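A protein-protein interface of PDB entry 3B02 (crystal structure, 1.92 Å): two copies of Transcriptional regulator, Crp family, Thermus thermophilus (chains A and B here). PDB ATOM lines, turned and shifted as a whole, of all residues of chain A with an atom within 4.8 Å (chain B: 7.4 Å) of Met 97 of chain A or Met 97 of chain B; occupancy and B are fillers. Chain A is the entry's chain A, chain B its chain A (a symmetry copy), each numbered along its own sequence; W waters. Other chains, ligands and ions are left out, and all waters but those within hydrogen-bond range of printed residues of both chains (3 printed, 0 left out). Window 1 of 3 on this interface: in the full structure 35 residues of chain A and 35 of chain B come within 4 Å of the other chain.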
ATOM      1  N   ARG A  43      -2.977 -25.749  -2.978  1.00  0.00           N
ATOM      2  CA  ARG A  43      -2.784 -24.321  -2.748  1.00  0.00           C
ATOM      3  C   ARG A  43      -2.366 -24.053  -1.306  1.00  0.00           C
ATOM      4  O   ARG A  43      -2.508 -24.915  -0.435  1.00  0.00           O
ATOM      5  CB  ARG A  43      -4.044 -23.501  -3.106  1.00  0.00           C
ATOM      6  CG  ARG A  43      -5.128 -23.374  -2.032  1.00  0.00           C
ATOM      7  CD  ARG A  43      -6.271 -22.484  -2.564  1.00  0.00           C
ATOM      8  NE  ARG A  43      -7.151 -21.942  -1.527  1.00  0.00           N
ATOM      9  CZ  ARG A  43      -8.232 -22.551  -1.045  1.00  0.00           C
ATOM     10  NH1 ARG A  43      -8.597 -23.753  -1.493  1.00  0.00           N
ATOM     11  NH2 ARG A  43      -8.970 -21.938  -0.130  1.00  0.00           N
ATOM     12  N   GLU A  53     -13.900 -23.428   1.470  1.00  0.00           N
ATOM     13  CA  GLU A  53     -14.758 -22.706   0.523  1.00  0.00           C
ATOM     14  C   GLU A  53     -15.991 -23.487   0.053  1.00  0.00           C
ATOM     15  O   GLU A  53     -17.001 -22.891  -0.342  1.00  0.00           O
ATOM     16  CB  GLU A  53     -13.931 -22.252  -0.706  1.00  0.00           C
ATOM     17  CG  GLU A  53     -13.239 -23.375  -1.506  1.00  0.00           C
ATOM     18  CD  GLU A  53     -11.934 -23.881  -0.894  1.00  0.00           C
ATOM     19  OE1 GLU A  53     -11.516 -23.364   0.160  1.00  0.00           O
ATOM     20  OE2 GLU A  53     -11.315 -24.804  -1.478  1.00  0.00           O
ATOM     21  N   LEU A  93     -11.278 -14.336  -2.107  1.00  0.00           N
ATOM     22  CA  LEU A  93     -11.326 -15.501  -2.987  1.00  0.00           C
ATOM     23  C   LEU A  93     -10.700 -15.125  -4.328  1.00  0.00           C
ATOM     24  O   LEU A  93     -10.037 -15.943  -4.961  1.00  0.00           O
ATOM     25  CB  LEU A  93     -12.767 -15.987  -3.184  1.00  0.00           C
ATOM     26  CG  LEU A  93     -13.316 -16.762  -1.976  1.00  0.00           C
ATOM     27  CD1 LEU A  93     -14.752 -17.229  -2.220  1.00  0.00           C
ATOM     28  CD2 LEU A  93     -12.417 -17.960  -1.734  1.00  0.00           C
ATOM     29  N   ALA A  94     -10.901 -13.882  -4.757  1.00  0.00           N
ATOM     30  CA  ALA A  94     -10.309 -13.432  -6.018  1.00  0.00           C
ATOM     31  C   ALA A  94      -8.781 -13.441  -5.893  1.00  0.00           C
ATOM     32  O   ALA A  94      -8.063 -13.804  -6.836  1.00  0.00           O
ATOM     33  CB  ALA A  94     -10.808 -12.039  -6.361  1.00  0.00           C
ATOM     34  N   ARG A  95      -8.272 -13.025  -4.736  1.00  0.00           N
ATOM     35  CA  ARG A  95      -6.823 -13.030  -4.538  1.00  0.00           C
ATOM     36  C   ARG A  95      -6.307 -14.460  -4.505  1.00  0.00           C
ATOM     37  O   ARG A  95      -5.251 -14.748  -5.051  1.00  0.00           O
ATOM     38  CB  ARG A  95      -6.442 -12.306  -3.240  1.00  0.00           C
ATOM     39  CG  ARG A  95      -6.564 -10.800  -3.353  1.00  0.00           C
ATOM     40  CD  ARG A  95      -6.218 -10.097  -2.060  1.00  0.00           C
ATOM     41  NE  ARG A  95      -6.335  -8.650  -2.213  1.00  0.00           N
ATOM     42  CZ  ARG A  95      -6.699  -7.819  -1.242  1.00  0.00           C
ATOM     43  NH1 ARG A  95      -6.988  -8.287  -0.035  1.00  0.00           N
ATOM     44  NH2 ARG A  95      -6.780  -6.516  -1.481  1.00  0.00           N
ATOM     45  N   GLN A  96      -7.039 -15.370  -3.865  1.00  0.00           N
ATOM     46  CA  GLN A  96      -6.561 -16.747  -3.846  1.00  0.00           C
ATOM     47  C   GLN A  96      -6.615 -17.376  -5.242  1.00  0.00           C
ATOM     48  O   GLN A  96      -5.800 -18.233  -5.575  1.00  0.00           O
ATOM     49  CB  GLN A  96      -7.366 -17.591  -2.862  1.00  0.00           C
ATOM     50  CG  GLN A  96      -7.193 -17.173  -1.410  1.00  0.00           C
ATOM     51  CD  GLN A  96      -7.870 -18.153  -0.467  1.00  0.00           C
ATOM     52  OE1 GLN A  96      -7.420 -19.286  -0.323  1.00  0.00           O
ATOM     53  NE2 GLN A  96      -8.965 -17.726   0.155  1.00  0.00           N
ATOM     54  N   MET A  97      -7.579 -16.957  -6.061  1.00  0.00           N
ATOM     55  CA  MET A  97      -7.681 -17.486  -7.428  1.00  0.00           C
ATOM     56  C   MET A  97      -6.444 -17.025  -8.210  1.00  0.00           C
ATOM     57  O   MET A  97      -5.861 -17.785  -8.996  1.00  0.00           O
ATOM     58  CB  MET A  97      -8.952 -16.958  -8.114  1.00  0.00           C
ATOM     59  CG  MET A  97      -9.109 -17.388  -9.576  1.00  0.00           C
ATOM     60  SD  MET A  97      -9.233 -19.182  -9.796  1.00  0.00           S
ATOM     61  CE  MET A  97     -10.395 -19.589  -8.391  1.00  0.00           C
ATOM     62  N   ARG A  98      -6.045 -15.778  -8.006  1.00  0.00           N
ATOM     63  CA  ARG A  98      -4.861 -15.275  -8.699  1.00  0.00           C
ATOM     64  C   ARG A  98      -3.634 -16.081  -8.265  1.00  0.00           C
ATOM     65  O   ARG A  98      -2.820 -16.488  -9.095  1.00  0.00           O
ATOM     66  CB  ARG A  98      -4.631 -13.784  -8.410  1.00  0.00           C
ATOM     67  CG  ARG A  98      -3.298 -13.277  -8.968  1.00  0.00           C
ATOM     68  CD  ARG A  98      -3.227 -11.760  -8.991  1.00  0.00           C
ATOM     69  NE  ARG A  98      -3.569 -11.170  -7.703  1.00  0.00           N
ATOM     70  CZ  ARG A  98      -2.837 -11.283  -6.601  1.00  0.00           C
ATOM     71  NH1 ARG A  98      -1.701 -11.975  -6.614  1.00  0.00           N
ATOM     72  NH2 ARG A  98      -3.239 -10.691  -5.484  1.00  0.00           N
ATOM     73  N   ARG A  99      -3.518 -16.331  -6.964  1.00  0.00           N
ATOM     74  CA  ARG A  99      -2.384 -17.071  -6.429  1.00  0.00           C
ATOM     75  C   ARG A  99      -2.337 -18.541  -6.825  1.00  0.00           C
ATOM     76  O   ARG A  99      -1.257 -19.077  -7.127  1.00  0.00           O
ATOM     77  CB  ARG A  99      -2.349 -16.913  -4.895  1.00  0.00           C
ATOM     78  CG  ARG A  99      -1.799 -15.531  -4.479  1.00  0.00           C
ATOM     79  CD  ARG A  99      -2.260 -15.095  -3.093  1.00  0.00           C
ATOM     80  NE  ARG A  99      -2.169 -16.180  -2.132  1.00  0.00           N
ATOM     81  CZ  ARG A  99      -2.940 -16.273  -1.055  1.00  0.00           C
ATOM     82  NH1 ARG A  99      -3.842 -15.332  -0.799  1.00  0.00           N
ATOM     83  NH2 ARG A  99      -2.846 -17.330  -0.269  1.00  0.00           N
ATOM     84  N   VAL A 100      -3.488 -19.205  -6.860  1.00  0.00           N
ATOM     85  CA  VAL A 100      -3.461 -20.614  -7.217  1.00  0.00           C
ATOM     86  C   VAL A 100      -3.159 -20.804  -8.696  1.00  0.00           C
ATOM     87  O   VAL A 100      -2.554 -21.798  -9.086  1.00  0.00           O
ATOM     88  CB  VAL A 100      -4.783 -21.353  -6.814  1.00  0.00           C
ATOM     89  CG1 VAL A 100      -5.935 -20.950  -7.715  1.00  0.00           C
ATOM     90  CG2 VAL A 100      -4.553 -22.863  -6.859  1.00  0.00           C
ATOM     91  N   GLN A 101      -3.560 -19.849  -9.526  1.00  0.00           N
ATOM     92  CA  GLN A 101      -3.264 -19.984 -10.949  1.00  0.00           C
ATOM     93  C   GLN A 101      -1.764 -19.756 -11.170  1.00  0.00           C
ATOM     94  O   GLN A 101      -1.139 -20.400 -12.013  1.00  0.00           O
ATOM     95  CB  GLN A 101      -4.115 -19.005 -11.752  1.00  0.00           C
ATOM     96  CG  GLN A 101      -5.574 -19.453 -11.803  1.00  0.00           C
ATOM     97  CD  GLN A 101      -6.478 -18.457 -12.485  1.00  0.00           C
ATOM     98  OE1 GLN A 101      -7.106 -18.770 -13.496  1.00  0.00           O
ATOM     99  NE2 GLN A 101      -6.550 -17.247 -11.938  1.00  0.00           N
ATOM    100  N   LEU B  42      -4.873 -22.092 -17.636  1.00  0.00           N
ATOM    101  CA  LEU B  42      -4.923 -22.072 -16.170  1.00  0.00           C
ATOM    102  C   LEU B  42      -6.264 -22.551 -15.617  1.00  0.00           C
ATOM    103  O   LEU B  42      -6.314 -23.202 -14.568  1.00  0.00           O
ATOM    104  CB  LEU B  42      -4.612 -20.663 -15.656  1.00  0.00           C
ATOM    105  CG  LEU B  42      -3.222 -20.182 -16.096  1.00  0.00           C
ATOM    106  CD1 LEU B  42      -3.080 -18.717 -15.751  1.00  0.00           C
ATOM    107  CD2 LEU B  42      -2.127 -21.014 -15.433  1.00  0.00           C
ATOM    108  N   ARG B  43      -7.350 -22.208 -16.304  1.00  0.00           N
ATOM    109  CA  ARG B  43      -8.679 -22.663 -15.903  1.00  0.00           C
ATOM    110  C   ARG B  43      -9.698 -22.414 -17.009  1.00  0.00           C
ATOM    111  O   ARG B  43      -9.445 -21.647 -17.943  1.00  0.00           O
ATOM    112  CB  ARG B  43      -9.145 -22.001 -14.585  1.00  0.00           C
ATOM    113  CG  ARG B  43      -9.810 -20.627 -14.686  1.00  0.00           C
ATOM    114  CD  ARG B  43     -10.242 -20.166 -13.278  1.00  0.00           C
ATOM    115  NE  ARG B  43     -11.241 -19.095 -13.268  1.00  0.00           N
ATOM    116  CZ  ARG B  43     -10.968 -17.792 -13.301  1.00  0.00           C
ATOM    117  NH1 ARG B  43      -9.707 -17.360 -13.352  1.00  0.00           N
ATOM    118  NH2 ARG B  43     -11.963 -16.917 -13.253  1.00  0.00           N
ATOM    119  N   TYR B  50     -17.785 -15.985 -13.018  1.00  0.00           N
ATOM    120  CA  TYR B  50     -17.258 -14.633 -12.999  1.00  0.00           C
ATOM    121  C   TYR B  50     -15.770 -14.750 -13.312  1.00  0.00           C
ATOM    122  O   TYR B  50     -15.107 -15.680 -12.851  1.00  0.00           O
ATOM    123  CB  TYR B  50     -17.431 -14.015 -11.614  1.00  0.00           C
ATOM    124  CG  TYR B  50     -18.866 -13.692 -11.299  1.00  0.00           C
ATOM    125  CD1 TYR B  50     -19.435 -12.489 -11.717  1.00  0.00           C
ATOM    126  CD2 TYR B  50     -19.680 -14.620 -10.640  1.00  0.00           C
ATOM    127  CE1 TYR B  50     -20.781 -12.212 -11.492  1.00  0.00           C
ATOM    128  CE2 TYR B  50     -21.028 -14.358 -10.409  1.00  0.00           C
ATOM    129  CZ  TYR B  50     -21.571 -13.151 -10.840  1.00  0.00           C
ATOM    130  OH  TYR B  50     -22.906 -12.896 -10.637  1.00  0.00           O
ATOM    131  N   GLU B  53     -11.472 -11.619 -12.384  1.00  0.00           N
ATOM    132  CA  GLU B  53     -11.543 -11.542 -10.918  1.00  0.00           C
ATOM    133  C   GLU B  53     -10.605 -10.509 -10.283  1.00  0.00           C
ATOM    134  O   GLU B  53     -10.867 -10.013  -9.181  1.00  0.00           O
ATOM    135  CB  GLU B  53     -11.275 -12.936 -10.299  1.00  0.00           C
ATOM    136  CG  GLU B  53      -9.912 -13.577 -10.642  1.00  0.00           C
ATOM    137  CD  GLU B  53      -9.849 -14.244 -12.014  1.00  0.00           C
ATOM    138  OE1 GLU B  53     -10.867 -14.248 -12.735  1.00  0.00           O
ATOM    139  OE2 GLU B  53      -8.774 -14.777 -12.375  1.00  0.00           O
ATOM    140  N   GLU B  54      -9.525 -10.179 -10.983  1.00  0.00           N
ATOM    141  CA  GLU B  54      -8.562  -9.194 -10.483  1.00  0.00           C
ATOM    142  C   GLU B  54      -9.232  -7.845 -10.210  1.00  0.00           C
ATOM    143  O   GLU B  54      -8.764  -7.064  -9.377  1.00  0.00           O
ATOM    144  CB  GLU B  54      -7.428  -9.009 -11.492  1.00  0.00           C
ATOM    145  CG  GLU B  54      -6.637 -10.278 -11.763  1.00  0.00           C
ATOM    146  CD  GLU B  54      -7.142 -11.039 -12.975  1.00  0.00           C
ATOM    147  OE1 GLU B  54      -8.374 -11.101 -13.170  1.00  0.00           O
ATOM    148  OE2 GLU B  54      -6.305 -11.581 -13.729  1.00  0.00           O
ATOM    149  N   GLU B  57      -9.833  -7.269  -6.609  1.00  0.00           N
ATOM    150  CA  GLU B  57      -8.720  -7.146  -5.675  1.00  0.00           C
ATOM    151  C   GLU B  57      -7.517  -6.306  -6.065  1.00  0.00           C
ATOM    152  O   GLU B  57      -6.913  -5.669  -5.204  1.00  0.00           O
ATOM    153  CB  GLU B  57      -8.235  -8.554  -5.298  1.00  0.00           C
ATOM    154  CG  GLU B  57      -7.810  -9.460  -6.473  1.00  0.00           C
ATOM    155  CD  GLU B  57      -6.342  -9.324  -6.853  1.00  0.00           C
ATOM    156  OE1 GLU B  57      -5.544  -8.881  -6.000  1.00  0.00           O
ATOM    157  OE2 GLU B  57      -5.978  -9.679  -8.001  1.00  0.00           O
ATOM    158  N   TYR B  63      -3.662 -12.371 -15.781  1.00  0.00           N
ATOM    159  CA  TYR B  63      -3.675 -13.369 -16.847  1.00  0.00           C
ATOM    160  C   TYR B  63      -4.475 -12.843 -18.041  1.00  0.00           C
ATOM    161  O   TYR B  63      -5.047 -11.752 -17.995  1.00  0.00           O
ATOM    162  CB  TYR B  63      -4.306 -14.675 -16.345  1.00  0.00           C
ATOM    163  CG  TYR B  63      -3.687 -15.174 -15.065  1.00  0.00           C
ATOM    164  CD1 TYR B  63      -2.405 -15.724 -15.057  1.00  0.00           C
ATOM    165  CD2 TYR B  63      -4.340 -14.992 -13.843  1.00  0.00           C
ATOM    166  CE1 TYR B  63      -1.781 -16.075 -13.858  1.00  0.00           C
ATOM    167  CE2 TYR B  63      -3.731 -15.338 -12.640  1.00  0.00           C
ATOM    168  CZ  TYR B  63      -2.448 -15.874 -12.656  1.00  0.00           C
ATOM    169  OH  TYR B  63      -1.827 -16.166 -11.461  1.00  0.00           O
ATOM    170  N   ARG B  91     -20.243 -17.370  -3.941  1.00  0.00           N
ATOM    171  CA  ARG B  91     -20.561 -18.763  -4.203  1.00  0.00           C
ATOM    172  C   ARG B  91     -19.912 -19.264  -5.486  1.00  0.00           C
ATOM    173  O   ARG B  91     -19.371 -20.373  -5.526  1.00  0.00           O
ATOM    174  CB  ARG B  91     -22.073 -18.976  -4.283  1.00  0.00           C
ATOM    175  CG  ARG B  91     -22.442 -20.345  -4.840  1.00  0.00           C
ATOM    176  CD  ARG B  91     -23.917 -20.694  -4.624  1.00  0.00           C
ATOM    177  NE  ARG B  91     -24.147 -21.229  -3.282  1.00  0.00           N
ATOM    178  CZ  ARG B  91     -25.258 -21.859  -2.903  1.00  0.00           C
ATOM    179  NH1 ARG B  91     -26.252 -22.036  -3.764  1.00  0.00           N
ATOM    180  NH2 ARG B  91     -25.372 -22.322  -1.663  1.00  0.00           N
ATOM    181  N   ASN B  92     -19.973 -18.459  -6.543  1.00  0.00           N
ATOM    182  CA  ASN B  92     -19.384 -18.876  -7.811  1.00  0.00           C
ATOM    183  C   ASN B  92     -17.854 -18.961  -7.779  1.00  0.00           C
ATOM    184  O   ASN B  92     -17.254 -19.854  -8.402  1.00  0.00           O
ATOM    185  CB  ASN B  92     -19.825 -17.952  -8.949  1.00  0.00           C
ATOM    186  CG  ASN B  92     -19.220 -18.367 -10.267  1.00  0.00           C
ATOM    187  OD1 ASN B  92     -18.263 -17.763 -10.735  1.00  0.00           O
ATOM    188  ND2 ASN B  92     -19.752 -19.438 -10.855  1.00  0.00           N
ATOM    189  N   LEU B  93     -17.212 -18.033  -7.070  1.00  0.00           N
ATOM    190  CA  LEU B  93     -15.755 -18.078  -6.975  1.00  0.00           C
ATOM    191  C   LEU B  93     -15.355 -19.335  -6.203  1.00  0.00           C
ATOM    192  O   LEU B  93     -14.340 -19.956  -6.504  1.00  0.00           O
ATOM    193  CB  LEU B  93     -15.209 -16.825  -6.280  1.00  0.00           C
ATOM    194  CG  LEU B  93     -15.203 -15.584  -7.186  1.00  0.00           C
ATOM    195  CD1 LEU B  93     -14.647 -14.362  -6.453  1.00  0.00           C
ATOM    196  CD2 LEU B  93     -14.351 -15.888  -8.402  1.00  0.00           C
ATOM    197  N   ALA B  94     -16.160 -19.714  -5.215  1.00  0.00           N
ATOM    198  CA  ALA B  94     -15.866 -20.925  -4.448  1.00  0.00           C
ATOM    199  C   ALA B  94     -15.961 -22.147  -5.369  1.00  0.00           C
ATOM    200  O   ALA B  94     -15.160 -23.086  -5.273  1.00  0.00           O
ATOM    201  CB  ALA B  94     -16.836 -21.057  -3.287  1.00  0.00           C
ATOM    202  N   ARG B  95     -16.951 -22.150  -6.260  1.00  0.00           N
ATOM    203  CA  ARG B  95     -17.088 -23.270  -7.188  1.00  0.00           C
ATOM    204  C   ARG B  95     -15.916 -23.289  -8.159  1.00  0.00           C
ATOM    205  O   ARG B  95     -15.401 -24.348  -8.487  1.00  0.00           O
ATOM    206  CB  ARG B  95     -18.408 -23.187  -7.963  1.00  0.00           C
ATOM    207  CG  ARG B  95     -19.608 -23.560  -7.114  1.00  0.00           C
ATOM    208  CD  ARG B  95     -20.909 -23.443  -7.876  1.00  0.00           C
ATOM    209  NE  ARG B  95     -22.038 -23.822  -7.031  1.00  0.00           N
ATOM    210  CZ  ARG B  95     -23.253 -23.296  -7.122  1.00  0.00           C
ATOM    211  NH1 ARG B  95     -23.510 -22.358  -8.025  1.00  0.00           N
ATOM    212  NH2 ARG B  95     -24.215 -23.704  -6.302  1.00  0.00           N
ATOM    213  N   GLN B  96     -15.485 -22.120  -8.631  1.00  0.00           N
ATOM    214  CA  GLN B  96     -14.352 -22.128  -9.549  1.00  0.00           C
ATOM    215  C   GLN B  96     -13.063 -22.557  -8.839  1.00  0.00           C
ATOM    216  O   GLN B  96     -12.182 -23.155  -9.450  1.00  0.00           O
ATOM    217  CB  GLN B  96     -14.160 -20.756 -10.191  1.00  0.00           C
ATOM    218  CG  GLN B  96     -15.304 -20.340 -11.102  1.00  0.00           C
ATOM    219  CD  GLN B  96     -14.980 -19.059 -11.849  1.00  0.00           C
ATOM    220  OE1 GLN B  96     -14.116 -19.051 -12.723  1.00  0.00           O
ATOM    221  NE2 GLN B  96     -15.651 -17.968 -11.488  1.00  0.00           N
ATOM    222  N   MET B  97     -12.948 -22.249  -7.548  1.00  0.00           N
ATOM    223  CA  MET B  97     -11.758 -22.652  -6.786  1.00  0.00           C
ATOM    224  C   MET B  97     -11.747 -24.185  -6.697  1.00  0.00           C
ATOM    225  O   MET B  97     -10.696 -24.827  -6.821  1.00  0.00           O
ATOM    226  CB  MET B  97     -11.799 -22.054  -5.370  1.00  0.00           C
ATOM    227  CG  MET B  97     -10.639 -22.484  -4.465  1.00  0.00           C
ATOM    228  SD  MET B  97      -9.011 -21.981  -5.081  1.00  0.00           S
ATOM    229  CE  MET B  97      -9.409 -20.236  -5.619  1.00  0.00           C
ATOM    230  N   ARG B  98     -12.913 -24.772  -6.475  1.00  0.00           N
ATOM    231  CA  ARG B  98     -12.984 -26.230  -6.402  1.00  0.00           C
ATOM    232  C   ARG B  98     -12.572 -26.831  -7.748  1.00  0.00           C
ATOM    233  O   ARG B  98     -11.797 -27.787  -7.801  1.00  0.00           O
ATOM    234  CB  ARG B  98     -14.398 -26.706  -6.031  1.00  0.00           C
ATOM    235  CG  ARG B  98     -14.550 -28.226  -6.131  1.00  0.00           C
ATOM    236  CD  ARG B  98     -15.812 -28.721  -5.446  1.00  0.00           C
ATOM    237  NE  ARG B  98     -17.000 -28.000  -5.882  1.00  0.00           N
ATOM    238  CZ  ARG B  98     -17.520 -28.068  -7.102  1.00  0.00           C
ATOM    239  NH1 ARG B  98     -16.957 -28.833  -8.033  1.00  0.00           N
ATOM    240  NH2 ARG B  98     -18.614 -27.374  -7.385  1.00  0.00           N
ATOM    241  N   ARG B  99     -13.072 -26.250  -8.834  1.00  0.00           N
ATOM    242  CA  ARG B  99     -12.769 -26.746 -10.170  1.00  0.00           C
ATOM    243  C   ARG B  99     -11.320 -26.559 -10.604  1.00  0.00           C
ATOM    244  O   ARG B  99     -10.731 -27.454 -11.231  1.00  0.00           O
ATOM    245  CB  ARG B  99     -13.735 -26.104 -11.185  1.00  0.00           C
ATOM    246  CG  ARG B  99     -15.134 -26.758 -11.129  1.00  0.00           C
ATOM    247  CD  ARG B  99     -16.244 -25.847 -11.641  1.00  0.00           C
ATOM    248  NE  ARG B  99     -15.858 -25.169 -12.867  1.00  0.00           N
ATOM    249  CZ  ARG B  99     -16.348 -23.996 -13.243  1.00  0.00           C
ATOM    250  NH1 ARG B  99     -17.256 -23.383 -12.492  1.00  0.00           N
ATOM    251  NH2 ARG B  99     -15.890 -23.411 -14.336  1.00  0.00           N
ATOM    252  N   VAL B 100     -10.720 -25.423 -10.264  1.00  0.00           N
ATOM    253  CA  VAL B 100      -9.343 -25.218 -10.688  1.00  0.00           C
ATOM    254  C   VAL B 100      -8.387 -26.108  -9.909  1.00  0.00           C
ATOM    255  O   VAL B 100      -7.354 -26.520 -10.429  1.00  0.00           O
ATOM    256  CB  VAL B 100      -8.913 -23.715 -10.595  1.00  0.00           C
ATOM    257  CG1 VAL B 100      -8.736 -23.280  -9.151  1.00  0.00           C
ATOM    258  CG2 VAL B 100      -7.626 -23.504 -11.393  1.00  0.00           C
ATOM    259  N   GLN B 101      -8.727 -26.426  -8.665  1.00  0.00           N
ATOM    260  CA  GLN B 101      -7.847 -27.302  -7.898  1.00  0.00           C
ATOM    261  C   GLN B 101      -7.951 -28.727  -8.452  1.00  0.00           C
ATOM    262  O   GLN B 101      -6.966 -29.465  -8.505  1.00  0.00           O
ATOM    263  CB  GLN B 101      -8.212 -27.236  -6.417  1.00  0.00           C
ATOM    264  CG  GLN B 101      -7.775 -25.910  -5.799  1.00  0.00           C
ATOM    265  CD  GLN B 101      -8.220 -25.749  -4.365  1.00  0.00           C
ATOM    266  OE1 GLN B 101      -7.394 -25.608  -3.465  1.00  0.00           O
ATOM    267  NE2 GLN B 101      -9.531 -25.773  -4.144  1.00  0.00           N
ATOM    268  N   ALA B 102      -9.150 -29.103  -8.887  1.00  0.00           N
ATOM    269  CA  ALA B 102      -9.340 -30.427  -9.478  1.00  0.00           C
ATOM    270  C   ALA B 102      -8.588 -30.489 -10.809  1.00  0.00           C
ATOM    271  O   ALA B 102      -8.039 -31.526 -11.179  1.00  0.00           O
ATOM    272  CB  ALA B 102     -10.801 -30.685  -9.710  1.00  0.00           C
ATOM    273  N   TYR B 103      -8.577 -29.370 -11.529  1.00  0.00           N
ATOM    274  CA  TYR B 103      -7.883 -29.299 -12.814  1.00  0.00           C
ATOM    275  C   TYR B 103      -6.381 -29.477 -12.570  1.00  0.00           C
ATOM    276  O   TYR B 103      -5.690 -30.209 -13.286  1.00  0.00           O
ATOM    277  CB  TYR B 103      -8.188 -27.953 -13.474  1.00  0.00           C
ATOM    278  CG  TYR B 103      -7.379 -27.671 -14.715  1.00  0.00           C
ATOM    279  CD1 TYR B 103      -7.445 -28.511 -15.826  1.00  0.00           C
ATOM    280  CD2 TYR B 103      -6.539 -26.559 -14.773  1.00  0.00           C
ATOM    281  CE1 TYR B 103      -6.686 -28.249 -16.976  1.00  0.00           C
ATOM    282  CE2 TYR B 103      -5.783 -26.284 -15.905  1.00  0.00           C
ATOM    283  CZ  TYR B 103      -5.859 -27.135 -17.003  1.00  0.00           C
ATOM    284  OH  TYR B 103      -5.093 -26.868 -18.115  1.00  0.00           O
ATOM    285  N   GLU B 104      -5.887 -28.794 -11.543  1.00  0.00           N
ATOM    286  CA  GLU B 104      -4.490 -28.885 -11.119  1.00  0.00           C
ATOM    287  C   GLU B 104      -4.091 -30.334 -10.877  1.00  0.00           C
ATOM    288  O   GLU B 104      -3.024 -30.785 -11.288  1.00  0.00           O
ATOM    289  CB  GLU B 104      -4.309 -28.213  -9.771  1.00  0.00           C
ATOM    290  CG  GLU B 104      -4.015 -26.785  -9.750  1.00  0.00           C
ATOM    291  CD  GLU B 104      -3.447 -26.428  -8.400  1.00  0.00           C
ATOM    292  OE1 GLU B 104      -4.219 -26.359  -7.422  1.00  0.00           O
ATOM    293  OE2 GLU B 104      -2.223 -26.252  -8.318  1.00  0.00           O
HETATM  294  O   HOH W   1      -7.436 -12.113  -8.910  1.00  0.00           O
HETATM  295  O   HOH W   2      -6.480 -13.940 -11.151  1.00  0.00           O
HETATM  296  O   HOH W   3     -12.734 -26.391  -3.188  1.00  0.00           O
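Arg 43 of chain A touches Met 97 of chain B, and with the chains exchanged Met 97 of chain A touches Arg 43 of chain B. Glu 53 of chain A touches Ala 94 of chain B, and with the chains exchanged Ala 94 of chain A touches Glu 53 of chain B. Glu 53 of chain A touches Met 97 of chain B, and with the chains exchanged Met 97 of chain A touches Glu 53 of chain B. 11 positions are printed for both chains. Of the 19 pairs that touch across the chains among the printed residues, 12 have their exchanged pair printed and touching as well.
Among the printed residues, pairs that only touch across the chains: Met 97 of chain A with Met 97 of chain B, Ala 94 of chain A with Glu 53 of chain B, Glu 53 of chain A with Ala 94 of chain B, Gln 101 of chain A with Tyr 63 of chain B, Val 100 of chain A with Glu 104 of chain B, Gln 101 of chain A with Leu 42 of chain B, Arg 43 of chain A with Met 97 of chain B, Met 97 of chain A with Arg 43 of chain B, Glu 53 of chain A with Met 97 of chain B, Met 97 of chain A with Glu 53 of chain B, Val 100 of chain A with Val 100 of chain B and Ala 94 of chain A with Glu 57 of chain B.
Of the printed residues of chain B, Met 97 of chain A touches Arg 43 (3.8 Å), Glu 53 (3.8 Å) and Met 97 (3.0 Å). Of the printed residues of chain A, Met 97 of chain B touches Arg 43 (3.8 Å), Glu 53 (3.8 Å) and Met 97 (3.0 Å). Of the printed residues of chain A, Glu 57 of chain B touches Ala 94 (3.96 Å), Arg 95 (3.4 Å) and Arg 98 (2.8 Å). Printed residues of chain B within 4 Å of Arg 95 of chain A: Glu 57 (3.4 Å). Asn 92 of chain B touches none of the printed residues of chain A. The nearest printed residue of chain B that does not touch Met 97 of chain A is Gln 96 of chain B (4.02 Å).
NH1 of Arg 43 of chain A lies within hydrogen-bond range of OE1 of Gln 101 of chain B, at 3.0 Å. OE2 of Glu 53 of chain A is in hydrogen-bond range of NE2 of Gln 101 of chain B, 3.4 Å away. The guanidinium group (NE) of Arg 95 of chain A is in salt-bridge range of the side-chain carboxylate (OE1) of Glu 57 of chain B, 3.9 Å away. The side-chain carboxylate (OE2) of Glu 57 of chain B lies within salt-bridge range of the guanidinium group (NE) of Arg 98 of chain A, at 2.8 Å. OH of Tyr 63 of chain B sits at hydrogen-bond distance from O of Arg 98 of chain A, 2.6 Å away. OE1 of Gln 101 of chain A is in hydrogen-bond range of NH1 of Arg 43 of chain B. The side-chain amide nitrogen of Gln 101 of chain A lies within hydrogen-bond range of the side-chain carboxylate of Glu 53 of chain B, at 3.4 Å.
Water W3 bridges OE2 of Glu 53 of chain A (2.7 Å) and NE2 of Gln 101 of chain B (3.4 Å). Water W2 lies within hydrogen-bond range of the side-chain carboxylate (OE2) of Glu 53 of chain B (2.7 Å), the side-chain amide nitrogen (NE2) of Gln 101 of chain A (3.4 Å) and the side-chain carboxylate (OE2) of Glu 54 of chain B (3.5 Å). Water W1 lies within hydrogen-bond range of the backbone carbonyl oxygen of Ala 94 of chain A (2.7 Å) and the side-chain carboxylate of Glu 57 of chain B (3.0 Å).
The guanidinium group (NH1) of Arg 43 of chain A is in salt-bridge range of the side-chain carboxylate (OE2) of Glu 53 of chain A (2.9 Å). The backbone carbonyl oxygen of Met 97 of chain A sits at hydrogen-bond distance from the side-chain amide nitrogen of Gln 101 of chain A, 3.1 Å away. The side-chain carboxylate of Glu 54 of chain B lies within hydrogen-bond range of the backbone NH of Tyr 63 of chain B (3.4 Å).
Hydrophobic or aromatic side chains of chain A within 4 Å of the printed part of chain B: Ala 94, Met 97 and Val 100. Hydrophobic or aromatic side chains of chain B within 4 Å of the printed part of chain A: Leu 42, Tyr 63, Ala 94, Met 97 and Val 100. Among the printed residues, 19 pairs touch across the chains. Among the printed residues, Asp or Glu carboxylates within 4 Å of a Lys or Arg side-chain nitrogen of the other chain: Arg 95 of chain A with Glu 57 of chain B (3.9 Å) and Arg 98 of chain A with Glu 57 of chain B (2.8 Å).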
